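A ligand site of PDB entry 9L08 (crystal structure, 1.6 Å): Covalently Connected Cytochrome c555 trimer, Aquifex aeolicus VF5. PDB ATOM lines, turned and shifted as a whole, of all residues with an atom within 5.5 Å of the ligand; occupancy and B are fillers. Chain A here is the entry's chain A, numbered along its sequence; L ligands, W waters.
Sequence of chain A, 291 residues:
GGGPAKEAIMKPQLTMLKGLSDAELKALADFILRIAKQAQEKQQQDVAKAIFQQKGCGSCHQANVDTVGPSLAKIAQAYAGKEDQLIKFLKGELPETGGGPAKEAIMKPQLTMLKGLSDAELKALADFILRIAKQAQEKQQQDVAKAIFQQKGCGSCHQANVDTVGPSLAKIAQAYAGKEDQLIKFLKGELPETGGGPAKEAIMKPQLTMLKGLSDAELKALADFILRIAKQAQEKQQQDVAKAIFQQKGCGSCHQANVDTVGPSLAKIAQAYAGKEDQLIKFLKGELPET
O3 of the ligand sits close to OE2 of Glu 96, at 3.3 Å. Merely in contact with the ligand: Pro 70 (3.4 Å), Val 68 (3.4 Å), Lys 103 (3.5 Å), Phe 89 (3.5 Å), Leu 86 (3.6 Å), Gln 110 (3.7 Å), Ile 75 (3.7 Å), Gly 98 (3.7 Å), Ile 106 (3.8 Å), Gly 69 (3.8 Å), Gly 56 (3.9 Å), Gly 99 (3.9 Å) and Leu 114 (3.9 Å). Hydrophobic or aromatic side chains within 4 Å of the ligand: His 61, Val 68, Pro 70, Ile 75, Tyr 79, Leu 86, Phe 89, Ile 106, Met 107 and Leu 114. Within 4 Å of the ligand: Gly 56, Cys 57, Cys 60, His 61, Val 68, Gly 69, Pro 70, Ile 75, Tyr 79, Leu 86, Phe 89, Glu 96, Thr 97, Gly 98, Gly 99, Lys 103, Glu 104, Ile 106, Met 107, Gln 110 and Leu 114.
O of Cys 60 is in hydrogen-bond range of N of Gly 69. A ring nitrogen (ND1) of His 61 lies within hydrogen-bond range of the backbone carbonyl oxygen (O) of Pro 70 (2.8 Å). OG of Ser 59 is in hydrogen-bond range of O of Gly 56 (2.9 Å). The backbone carbonyl oxygen of Phe 52 lies within hydrogen-bond range of the backbone NH of Cys 57.
The backbone NH (N) of Glu 104 lies within hydrogen-bond range of an oxygen (O3) of the ligand, 3.2 Å away. A carbon (C25) of the ligand is bonded to the side-chain sulfur of Cys 60 (1.8 Å). An oxygen (O2) of the ligand is in hydrogen-bond range of the backbone NH of Thr 97, 2.8 Å away. OG1 of Thr 97 lies within hydrogen-bond range of O1 of the ligand, at 2.8 Å. O2 of the ligand lies within hydrogen-bond range of OH of Tyr 79, at 2.7 Å. The side-chain sulfur (SG) of Cys 57 is bonded to a carbon (C18) of the ligand (1.8 Å). NE2 of His 61 is bound to FE1 of the ligand, at 2.0 Å. FE1 of the ligand is bound by SD of Met 107 (2.4 Å).
Water W2 lies within hydrogen-bond range of the backbone NH of Gly 98 (2.9 Å), an oxygen (O1) of the ligand (3.1 Å), the side-chain carboxylate of Glu 96 (3.1 Å) and the side-chain hydroxyl of Thr 97 (3.5 Å). Water W3 bridges O of Lys 55 (2.8 Å) and OE1 of Gln 110 (2.8 Å).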
ATOM      1  N   PHE A  52      12.285 -22.174 -19.586  1.00  0.00           N
ATOM      2  CA  PHE A  52      13.240 -21.082 -19.426  1.00  0.00           C
ATOM      3  C   PHE A  52      14.678 -21.572 -19.552  1.00  0.00           C
ATOM      4  O   PHE A  52      15.520 -20.916 -20.186  1.00  0.00           O
ATOM      5  CB  PHE A  52      12.997 -20.433 -18.062  1.00  0.00           C
ATOM      6  CG  PHE A  52      13.660 -19.101 -17.876  1.00  0.00           C
ATOM      7  CD1 PHE A  52      13.005 -17.928 -18.235  1.00  0.00           C
ATOM      8  CD2 PHE A  52      14.903 -19.011 -17.287  1.00  0.00           C
ATOM      9  CE1 PHE A  52      13.607 -16.695 -18.028  1.00  0.00           C
ATOM     10  CE2 PHE A  52      15.519 -17.780 -17.095  1.00  0.00           C
ATOM     11  CZ  PHE A  52      14.867 -16.621 -17.462  1.00  0.00           C
ATOM     12  N   LYS A  55      15.405 -23.071 -23.341  1.00  0.00           N
ATOM     13  CA  LYS A  55      15.499 -22.073 -24.393  1.00  0.00           C
ATOM     14  C   LYS A  55      16.653 -21.101 -24.180  1.00  0.00           C
ATOM     15  O   LYS A  55      16.906 -20.290 -25.070  1.00  0.00           O
ATOM     16  CB  LYS A  55      14.186 -21.300 -24.538  1.00  0.00           C
ATOM     17  CG  LYS A  55      12.958 -22.186 -24.804  1.00  0.00           C
ATOM     18  CD  LYS A  55      13.163 -23.121 -25.993  1.00  0.00           C
ATOM     19  CE  LYS A  55      11.863 -23.864 -26.317  1.00  0.00           C
ATOM     20  NZ  LYS A  55      12.061 -24.995 -27.253  1.00  0.00           N
ATOM     21  N   GLY A  56      17.330 -21.151 -23.034  1.00  0.00           N
ATOM     22  CA  GLY A  56      18.505 -20.321 -22.814  1.00  0.00           C
ATOM     23  C   GLY A  56      18.239 -18.922 -22.310  1.00  0.00           C
ATOM     24  O   GLY A  56      19.156 -18.087 -22.342  1.00  0.00           O
ATOM     25  N   CYS A  57      17.027 -18.638 -21.828  1.00  0.00           N
ATOM     26  CA  CYS A  57      16.656 -17.272 -21.423  1.00  0.00           C
ATOM     27  C   CYS A  57      17.538 -16.731 -20.309  1.00  0.00           C
ATOM     28  O   CYS A  57      17.761 -15.515 -20.232  1.00  0.00           O
ATOM     29  CB  CYS A  57      15.193 -17.229 -20.980  1.00  0.00           C
ATOM     30  SG  CYS A  57      14.074 -18.014 -22.146  1.00  0.00           S
ATOM     31  N   SER A  59      20.603 -16.817 -19.938  1.00  0.00           N
ATOM     32  CA  SER A  59      21.849 -16.237 -20.435  1.00  0.00           C
ATOM     33  C   SER A  59      21.864 -14.717 -20.272  1.00  0.00           C
ATOM     34  O   SER A  59      22.918 -14.118 -20.034  1.00  0.00           O
ATOM     35  CB  SER A  59      22.051 -16.591 -21.912  1.00  0.00           C
ATOM     36  OG  SER A  59      22.051 -17.993 -22.115  1.00  0.00           O
ATOM     37  N   CYS A  60      20.692 -14.083 -20.406  1.00  0.00           N
ATOM     38  CA  CYS A  60      20.576 -12.635 -20.350  1.00  0.00           C
ATOM     39  C   CYS A  60      19.605 -12.160 -19.286  1.00  0.00           C
ATOM     40  O   CYS A  60      19.439 -10.944 -19.129  1.00  0.00           O
ATOM     41  CB  CYS A  60      20.114 -12.087 -21.701  1.00  0.00           C
ATOM     42  SG  CYS A  60      21.196 -12.549 -23.063  1.00  0.00           S
ATOM     43  N   HIS A  61      18.941 -13.064 -18.578  1.00  0.00           N
ATOM     44  CA  HIS A  61      17.892 -12.700 -17.623  1.00  0.00           C
ATOM     45  C   HIS A  61      18.156 -13.428 -16.305  1.00  0.00           C
ATOM     46  O   HIS A  61      17.724 -14.567 -16.132  1.00  0.00           O
ATOM     47  CB  HIS A  61      16.505 -13.032 -18.174  1.00  0.00           C
ATOM     48  CG  HIS A  61      16.104 -12.188 -19.342  1.00  0.00           C
ATOM     49  ND1 HIS A  61      15.980 -10.820 -19.272  1.00  0.00           N
ATOM     50  CD2 HIS A  61      15.784 -12.534 -20.616  1.00  0.00           C
ATOM     51  CE1 HIS A  61      15.597 -10.350 -20.439  1.00  0.00           C
ATOM     52  NE2 HIS A  61      15.471 -11.365 -21.284  1.00  0.00           N
ATOM     53  N   VAL A  68      23.073  -8.646 -19.786  1.00  0.00           N
ATOM     54  CA  VAL A  68      22.765  -8.195 -21.145  1.00  0.00           C
ATOM     55  C   VAL A  68      21.307  -7.766 -21.242  1.00  0.00           C
ATOM     56  O   VAL A  68      20.970  -6.788 -21.914  1.00  0.00           O
ATOM     57  CB  VAL A  68      23.121  -9.293 -22.168  1.00  0.00           C
ATOM     58  CG1 VAL A  68      22.488  -8.991 -23.535  1.00  0.00           C
ATOM     59  CG2 VAL A  68      24.642  -9.400 -22.310  1.00  0.00           C
ATOM     60  N   GLY A  69      20.417  -8.483 -20.549  1.00  0.00           N
ATOM     61  CA  GLY A  69      19.028  -8.107 -20.475  1.00  0.00           C
ATOM     62  C   GLY A  69      18.621  -7.688 -19.080  1.00  0.00           C
ATOM     63  O   GLY A  69      19.369  -7.844 -18.107  1.00  0.00           O
ATOM     64  N   PRO A  70      17.421  -7.124 -18.953  1.00  0.00           N
ATOM     65  CA  PRO A  70      16.923  -6.730 -17.629  1.00  0.00           C
ATOM     66  C   PRO A  70      16.711  -7.929 -16.715  1.00  0.00           C
ATOM     67  O   PRO A  70      16.465  -9.053 -17.159  1.00  0.00           O
ATOM     68  CB  PRO A  70      15.580  -6.056 -17.948  1.00  0.00           C
ATOM     69  CG  PRO A  70      15.170  -6.676 -19.267  1.00  0.00           C
ATOM     70  CD  PRO A  70      16.449  -6.832 -20.019  1.00  0.00           C
ATOM     71  N   ILE A  75      11.484  -6.925 -15.341  1.00  0.00           N
ATOM     72  CA  ILE A  75      10.425  -7.347 -16.263  1.00  0.00           C
ATOM     73  C   ILE A  75       9.107  -7.467 -15.505  1.00  0.00           C
ATOM     74  O   ILE A  75       8.058  -7.020 -15.990  1.00  0.00           O
ATOM     75  CB  ILE A  75      10.805  -8.664 -16.958  1.00  0.00           C
ATOM     76  CG1 ILE A  75      12.019  -8.472 -17.867  1.00  0.00           C
ATOM     77  CG2 ILE A  75       9.621  -9.172 -17.783  1.00  0.00           C
ATOM     78  CD1 ILE A  75      12.587  -9.778 -18.408  1.00  0.00           C
ATOM     79  N   ALA A  78       7.624  -4.124 -15.078  1.00  0.00           N
ATOM     80  CA  ALA A  78       7.094  -3.559 -16.315  1.00  0.00           C
ATOM     81  C   ALA A  78       5.745  -4.149 -16.676  1.00  0.00           C
ATOM     82  O   ALA A  78       4.925  -3.481 -17.310  1.00  0.00           O
ATOM     83  CB  ALA A  78       8.087  -3.783 -17.467  1.00  0.00           C
ATOM     84  N   TYR A  79       5.480  -5.395 -16.284  1.00  0.00           N
ATOM     85  CA  TYR A  79       4.250  -6.085 -16.630  1.00  0.00           C
ATOM     86  C   TYR A  79       3.311  -6.260 -15.439  1.00  0.00           C
ATOM     87  O   TYR A  79       2.366  -7.051 -15.508  1.00  0.00           O
ATOM     88  CB  TYR A  79       4.566  -7.437 -17.272  1.00  0.00           C
ATOM     89  CG  TYR A  79       5.028  -7.298 -18.715  1.00  0.00           C
ATOM     90  CD1 TYR A  79       4.104  -7.101 -19.724  1.00  0.00           C
ATOM     91  CD2 TYR A  79       6.368  -7.362 -19.052  1.00  0.00           C
ATOM     92  CE1 TYR A  79       4.488  -6.972 -21.032  1.00  0.00           C
ATOM     93  CE2 TYR A  79       6.775  -7.216 -20.367  1.00  0.00           C
ATOM     94  CZ  TYR A  79       5.820  -7.030 -21.350  1.00  0.00           C
ATOM     95  OH  TYR A  79       6.168  -6.892 -22.679  1.00  0.00           O
ATOM     96  N   LEU A  86       1.985  -9.542 -21.260  1.00  0.00           N
ATOM     97  CA  LEU A  86       3.220 -10.320 -21.274  1.00  0.00           C
ATOM     98  C   LEU A  86       3.079 -11.545 -22.167  1.00  0.00           C
ATOM     99  O   LEU A  86       3.983 -11.867 -22.946  1.00  0.00           O
ATOM    100  CB  LEU A  86       3.601 -10.720 -19.849  1.00  0.00           C
ATOM    101  CG  LEU A  86       4.850 -11.596 -19.712  1.00  0.00           C
ATOM    102  CD1 LEU A  86       6.073 -10.970 -20.406  1.00  0.00           C
ATOM    103  CD2 LEU A  86       5.151 -11.855 -18.226  1.00  0.00           C
ATOM    104  N   PHE A  89       3.221 -10.386 -25.700  1.00  0.00           N
ATOM    105  CA  PHE A  89       4.600 -10.073 -26.053  1.00  0.00           C
ATOM    106  C   PHE A  89       5.389 -11.336 -26.383  1.00  0.00           C
ATOM    107  O   PHE A  89       6.127 -11.385 -27.382  1.00  0.00           O
ATOM    108  CB  PHE A  89       5.294  -9.296 -24.937  1.00  0.00           C
ATOM    109  CG  PHE A  89       6.767  -9.129 -25.183  1.00  0.00           C
ATOM    110  CD1 PHE A  89       7.235  -8.147 -26.049  1.00  0.00           C
ATOM    111  CD2 PHE A  89       7.695  -9.989 -24.591  1.00  0.00           C
ATOM    112  CE1 PHE A  89       8.579  -8.002 -26.307  1.00  0.00           C
ATOM    113  CE2 PHE A  89       9.039  -9.867 -24.846  1.00  0.00           C
ATOM    114  CZ  PHE A  89       9.493  -8.867 -25.714  1.00  0.00           C
ATOM    115  N   LEU A  90       5.238 -12.373 -25.551  1.00  0.00           N
ATOM    116  CA  LEU A  90       5.988 -13.602 -25.782  1.00  0.00           C
ATOM    117  C   LEU A  90       5.595 -14.286 -27.077  1.00  0.00           C
ATOM    118  O   LEU A  90       6.401 -15.030 -27.641  1.00  0.00           O
ATOM    119  CB  LEU A  90       5.795 -14.577 -24.605  1.00  0.00           C
ATOM    120  CG  LEU A  90       6.306 -14.159 -23.223  1.00  0.00           C
ATOM    121  CD1 LEU A  90       5.853 -15.129 -22.133  1.00  0.00           C
ATOM    122  CD2 LEU A  90       7.835 -14.033 -23.242  1.00  0.00           C
ATOM    123  N   PRO A  95       4.695  -4.791 -28.917  1.00  0.00           N
ATOM    124  CA  PRO A  95       6.054  -4.238 -28.852  1.00  0.00           C
ATOM    125  C   PRO A  95       6.597  -4.265 -27.434  1.00  0.00           C
ATOM    126  O   PRO A  95       5.874  -4.480 -26.448  1.00  0.00           O
ATOM    127  CB  PRO A  95       5.880  -2.810 -29.355  1.00  0.00           C
ATOM    128  CG  PRO A  95       4.480  -2.454 -28.981  1.00  0.00           C
ATOM    129  CD  PRO A  95       3.683  -3.733 -29.121  1.00  0.00           C
ATOM    130  N   GLU A  96       7.906  -4.081 -27.350  1.00  0.00           N
ATOM    131  CA  GLU A  96       8.582  -3.906 -26.062  1.00  0.00           C
ATOM    132  C   GLU A  96       7.956  -2.764 -25.280  1.00  0.00           C
ATOM    133  O   GLU A  96       7.511  -1.767 -25.849  1.00  0.00           O
ATOM    134  CB  GLU A  96      10.063  -3.604 -26.286  1.00  0.00           C
ATOM    135  CG  GLU A  96      10.831  -4.712 -26.975  1.00  0.00           C
ATOM    136  CD  GLU A  96      11.410  -5.698 -25.996  1.00  0.00           C
ATOM    137  OE1 GLU A  96      11.960  -6.726 -26.444  1.00  0.00           O
ATOM    138  OE2 GLU A  96      11.339  -5.455 -24.772  1.00  0.00           O
ATOM    139  N   THR A  97       7.932  -2.903 -23.955  1.00  0.00           N
ATOM    140  CA  THR A  97       7.367  -1.852 -23.118  1.00  0.00           C
ATOM    141  C   THR A  97       8.223  -0.594 -23.114  1.00  0.00           C
ATOM    142  O   THR A  97       7.710   0.488 -22.847  1.00  0.00           O
ATOM    143  CB  THR A  97       7.170  -2.343 -21.688  1.00  0.00           C
ATOM    144  OG1 THR A  97       8.423  -2.773 -21.145  1.00  0.00           O
ATOM    145  CG2 THR A  97       6.158  -3.487 -21.645  1.00  0.00           C
ATOM    146  N   GLY A  98       9.509  -0.719 -23.386  1.00  0.00           N
ATOM    147  CA  GLY A  98      10.408   0.426 -23.357  1.00  0.00           C
ATOM    148  C   GLY A  98      11.681   0.118 -24.099  1.00  0.00           C
ATOM    149  O   GLY A  98      11.711  -0.715 -24.992  1.00  0.00           O
ATOM    150  N   GLY A  99      12.739   0.818 -23.712  1.00  0.00           N
ATOM    151  CA  GLY A  99      14.034   0.617 -24.332  1.00  0.00           C
ATOM    152  C   GLY A  99      14.125   1.256 -25.714  1.00  0.00           C
ATOM    153  O   GLY A  99      13.171   1.825 -26.245  1.00  0.00           O
ATOM    154  N   GLY A 100      15.310   1.146 -26.297  1.00  0.00           N
ATOM    155  CA  GLY A 100      15.564   1.686 -27.606  1.00  0.00           C
ATOM    156  C   GLY A 100      15.711   0.581 -28.637  1.00  0.00           C
ATOM    157  O   GLY A 100      15.459  -0.590 -28.367  1.00  0.00           O
ATOM    158  N   LYS A 103      18.508  -2.516 -27.846  1.00  0.00           N
ATOM    159  CA  LYS A 103      18.016  -3.586 -26.994  1.00  0.00           C
ATOM    160  C   LYS A 103      16.906  -4.368 -27.689  1.00  0.00           C
ATOM    161  O   LYS A 103      16.817  -5.590 -27.535  1.00  0.00           O
ATOM    162  CB  LYS A 103      17.520  -3.019 -25.659  1.00  0.00           C
ATOM    163  CG  LYS A 103      18.599  -2.353 -24.814  1.00  0.00           C
ATOM    164  CD  LYS A 103      19.744  -3.294 -24.534  1.00  0.00           C
ATOM    165  CE  LYS A 103      20.875  -2.611 -23.766  1.00  0.00           C
ATOM    166  NZ  LYS A 103      21.975  -3.548 -23.419  1.00  0.00           N
ATOM    167  N   GLU A 104      16.067  -3.674 -28.471  1.00  0.00           N
ATOM    168  CA  GLU A 104      14.977  -4.359 -29.157  1.00  0.00           C
ATOM    169  C   GLU A 104      15.516  -5.416 -30.103  1.00  0.00           C
ATOM    170  O   GLU A 104      14.956  -6.516 -30.199  1.00  0.00           O
ATOM    171  CB  GLU A 104      14.124  -3.338 -29.917  1.00  0.00           C
ATOM    172  CG  GLU A 104      13.063  -3.959 -30.806  1.00  0.00           C
ATOM    173  CD  GLU A 104      12.425  -2.965 -31.745  1.00  0.00           C
ATOM    174  OE1 GLU A 104      12.838  -1.785 -31.774  1.00  0.00           O
ATOM    175  OE2 GLU A 104      11.488  -3.367 -32.466  1.00  0.00           O
ATOM    176  N   ILE A 106      18.345  -7.039 -29.844  1.00  0.00           N
ATOM    177  CA  ILE A 106      18.872  -8.187 -29.095  1.00  0.00           C
ATOM    178  C   ILE A 106      17.761  -9.170 -28.774  1.00  0.00           C
ATOM    179  O   ILE A 106      17.897 -10.387 -29.003  1.00  0.00           O
ATOM    180  CB  ILE A 106      19.581  -7.699 -27.807  1.00  0.00           C
ATOM    181  CG1 ILE A 106      20.842  -6.896 -28.159  1.00  0.00           C
ATOM    182  CG2 ILE A 106      19.929  -8.874 -26.921  1.00  0.00           C
ATOM    183  CD1 ILE A 106      21.573  -6.346 -26.955  1.00  0.00           C
ATOM    184  N   MET A 107      16.648  -8.678 -28.245  1.00  0.00           N
ATOM    185  CA  MET A 107      15.633  -9.586 -27.711  1.00  0.00           C
ATOM    186  C   MET A 107      14.707 -10.137 -28.784  1.00  0.00           C
ATOM    187  O   MET A 107      14.212 -11.259 -28.645  1.00  0.00           O
ATOM    188  CB  MET A 107      14.838  -8.868 -26.615  1.00  0.00           C
ATOM    189  CG  MET A 107      13.686  -9.693 -26.042  1.00  0.00           C
ATOM    190  SD  MET A 107      14.179 -11.335 -25.441  1.00  0.00           S
ATOM    191  CE  MET A 107      12.579 -12.192 -25.584  1.00  0.00           C
ATOM    192  N   GLN A 110      15.062 -13.744 -30.048  1.00  0.00           N
ATOM    193  CA  GLN A 110      14.855 -14.746 -29.008  1.00  0.00           C
ATOM    194  C   GLN A 110      13.381 -15.141 -28.881  1.00  0.00           C
ATOM    195  O   GLN A 110      13.089 -16.221 -28.351  1.00  0.00           O
ATOM    196  CB  GLN A 110      15.392 -14.242 -27.667  1.00  0.00           C
ATOM    197  CG  GLN A 110      16.870 -13.919 -27.728  1.00  0.00           C
ATOM    198  CD  GLN A 110      17.708 -15.140 -28.083  1.00  0.00           C
ATOM    199  OE1 GLN A 110      17.415 -16.246 -27.651  1.00  0.00           O
ATOM    200  NE2 GLN A 110      18.741 -14.935 -28.890  1.00  0.00           N
ATOM    201  N   MET A 113      12.374 -18.602 -30.076  1.00  0.00           N
ATOM    202  CA  MET A 113      12.507 -19.779 -29.233  1.00  0.00           C
ATOM    203  C   MET A 113      11.177 -20.248 -28.660  1.00  0.00           C
ATOM    204  O   MET A 113      11.088 -21.391 -28.207  1.00  0.00           O
ATOM    205  CB  MET A 113      13.482 -19.492 -28.084  1.00  0.00           C
ATOM    206  CG  MET A 113      14.865 -19.004 -28.522  1.00  0.00           C
ATOM    207  SD  MET A 113      15.790 -20.236 -29.465  1.00  0.00           S
ATOM    208  CE  MET A 113      15.722 -21.630 -28.346  1.00  0.00           C
ATOM    209  N   LEU A 114      10.157 -19.404 -28.667  1.00  0.00           N
ATOM    210  CA  LEU A 114       8.878 -19.721 -28.047  1.00  0.00           C
ATOM    211  C   LEU A 114       7.800 -20.095 -29.049  1.00  0.00           C
ATOM    212  O   LEU A 114       6.671 -20.350 -28.640  1.00  0.00           O
ATOM    213  CB  LEU A 114       8.409 -18.531 -27.201  1.00  0.00           C
ATOM    214  CG  LEU A 114       9.411 -18.036 -26.160  1.00  0.00           C
ATOM    215  CD1 LEU A 114       8.828 -16.834 -25.412  1.00  0.00           C
ATOM    216  CD2 LEU A 114       9.820 -19.132 -25.167  1.00  0.00           C
ATOM    217  N   LEU A 125       4.881 -19.917 -18.313  1.00  0.00           N
ATOM    218  CA  LEU A 125       6.121 -19.153 -18.443  1.00  0.00           C
ATOM    219  C   LEU A 125       5.928 -17.710 -18.027  1.00  0.00           C
ATOM    220  O   LEU A 125       6.785 -17.119 -17.362  1.00  0.00           O
ATOM    221  CB  LEU A 125       6.637 -19.235 -19.894  1.00  0.00           C
ATOM    222  CG  LEU A 125       7.938 -18.504 -20.185  1.00  0.00           C
ATOM    223  CD1 LEU A 125       9.074 -19.062 -19.352  1.00  0.00           C
ATOM    224  CD2 LEU A 125       8.244 -18.624 -21.684  1.00  0.00           C
ATOM    225  N   ILE A 129       7.860 -15.699 -15.043  1.00  0.00           N
ATOM    226  CA  ILE A 129       8.570 -14.434 -15.239  1.00  0.00           C
ATOM    227  C   ILE A 129       8.089 -13.379 -14.250  1.00  0.00           C
ATOM    228  O   ILE A 129       8.886 -12.579 -13.736  1.00  0.00           O
ATOM    229  CB  ILE A 129       8.400 -13.979 -16.703  1.00  0.00           C
ATOM    230  CG1 ILE A 129       9.192 -14.909 -17.626  1.00  0.00           C
ATOM    231  CG2 ILE A 129       8.822 -12.522 -16.850  1.00  0.00           C
ATOM    232  CD1 ILE A 129       8.893 -14.739 -19.101  1.00  0.00           C
HETATM  233 FE1  LIG L   1      14.855 -11.306 -23.170  1.00  0.00          FE
HETATM  234  C1  LIG L   1      13.593  -8.157 -22.716  1.00  0.00           C
HETATM  235  C2  LIG L   1      11.879 -12.629 -22.084  1.00  0.00           C
HETATM  236  C3  LIG L   1      15.963 -14.477 -23.968  1.00  0.00           C
HETATM  237  C4  LIG L   1      17.953 -10.049 -23.919  1.00  0.00           C
HETATM  238  N1  LIG L   1      13.076 -10.546 -22.564  1.00  0.00           N
HETATM  239  C5  LIG L   1      12.778  -9.209 -22.392  1.00  0.00           C
HETATM  240  C6  LIG L   1      11.451  -9.083 -21.824  1.00  0.00           C
HETATM  241  C7  LIG L   1      10.972 -10.328 -21.657  1.00  0.00           C
HETATM  242  C8  LIG L   1      11.979 -11.269 -22.115  1.00  0.00           C
HETATM  243  C9  LIG L   1       9.601 -10.750 -21.102  1.00  0.00           C
HETATM  244  C10 LIG L   1      10.799  -7.717 -21.498  1.00  0.00           C
HETATM  245  C11 LIG L   1       9.876  -7.306 -22.627  1.00  0.00           C
HETATM  246  C12 LIG L   1       9.338  -5.910 -22.403  1.00  0.00           C
HETATM  247  O1  LIG L   1       9.822  -5.184 -21.501  1.00  0.00           O
HETATM  248  O2  LIG L   1       8.396  -5.504 -23.129  1.00  0.00           O
HETATM  249  N2  LIG L   1      14.082 -13.190 -23.040  1.00  0.00           N
HETATM  250  C13 LIG L   1      12.818 -13.511 -22.559  1.00  0.00           C
HETATM  251  C14 LIG L   1      12.666 -14.941 -22.670  1.00  0.00           C
HETATM  252  C15 LIG L   1      13.792 -15.445 -23.184  1.00  0.00           C
HETATM  253  C16 LIG L   1      14.697 -14.345 -23.439  1.00  0.00           C
HETATM  254  C17 LIG L   1      11.393 -15.694 -22.209  1.00  0.00           C
HETATM  255  C18 LIG L   1      14.150 -16.901 -23.522  1.00  0.00           C
HETATM  256  C19 LIG L   1      13.249 -17.382 -24.690  1.00  0.00           C
HETATM  257  N3  LIG L   1      16.607 -12.114 -23.826  1.00  0.00           N
HETATM  258  C20 LIG L   1      16.876 -13.448 -24.039  1.00  0.00           C
HETATM  259  C21 LIG L   1      18.279 -13.589 -24.321  1.00  0.00           C
HETATM  260  C22 LIG L   1      18.833 -12.370 -24.314  1.00  0.00           C
HETATM  261  C23 LIG L   1      17.784 -11.411 -24.024  1.00  0.00           C
HETATM  262  C24 LIG L   1      18.945 -14.956 -24.591  1.00  0.00           C
HETATM  263  C25 LIG L   1      20.314 -11.960 -24.536  1.00  0.00           C
HETATM  264  C26 LIG L   1      20.907 -12.400 -25.887  1.00  0.00           C
HETATM  265  N4  LIG L   1      15.650  -9.437 -23.277  1.00  0.00           N
HETATM  266  C27 LIG L   1      16.954  -9.134 -23.660  1.00  0.00           C
HETATM  267  C28 LIG L   1      17.101  -7.711 -23.750  1.00  0.00           C
HETATM  268  C29 LIG L   1      15.754  -7.135 -23.362  1.00  0.00           C
HETATM  269  C30 LIG L   1      14.906  -8.263 -23.090  1.00  0.00           C
HETATM  270  C31 LIG L   1      18.350  -6.910 -24.142  1.00  0.00           C
HETATM  271  C32 LIG L   1      15.347  -5.661 -23.326  1.00  0.00           C
HETATM  272  C33 LIG L   1      14.727  -5.485 -24.694  1.00  0.00           C
HETATM  273  C34 LIG L   1      14.265  -4.085 -24.972  1.00  0.00           C
HETATM  274  O3  LIG L   1      13.843  -3.846 -26.140  1.00  0.00           O
HETATM  275  O4  LIG L   1      14.311  -3.226 -24.063  1.00  0.00           O
HETATM  276  O   HOH W   1      15.235  -2.560 -21.489  1.00  0.00           O
HETATM  277  O   HOH W   2      11.353  -2.980 -22.956  1.00  0.00           O
HETATM  278  O   HOH W   3      16.859 -17.543 -25.237  1.00  0.00           O
HETATM  279  O   HOH W   4      13.135  -1.478 -27.111  1.00  0.00           O
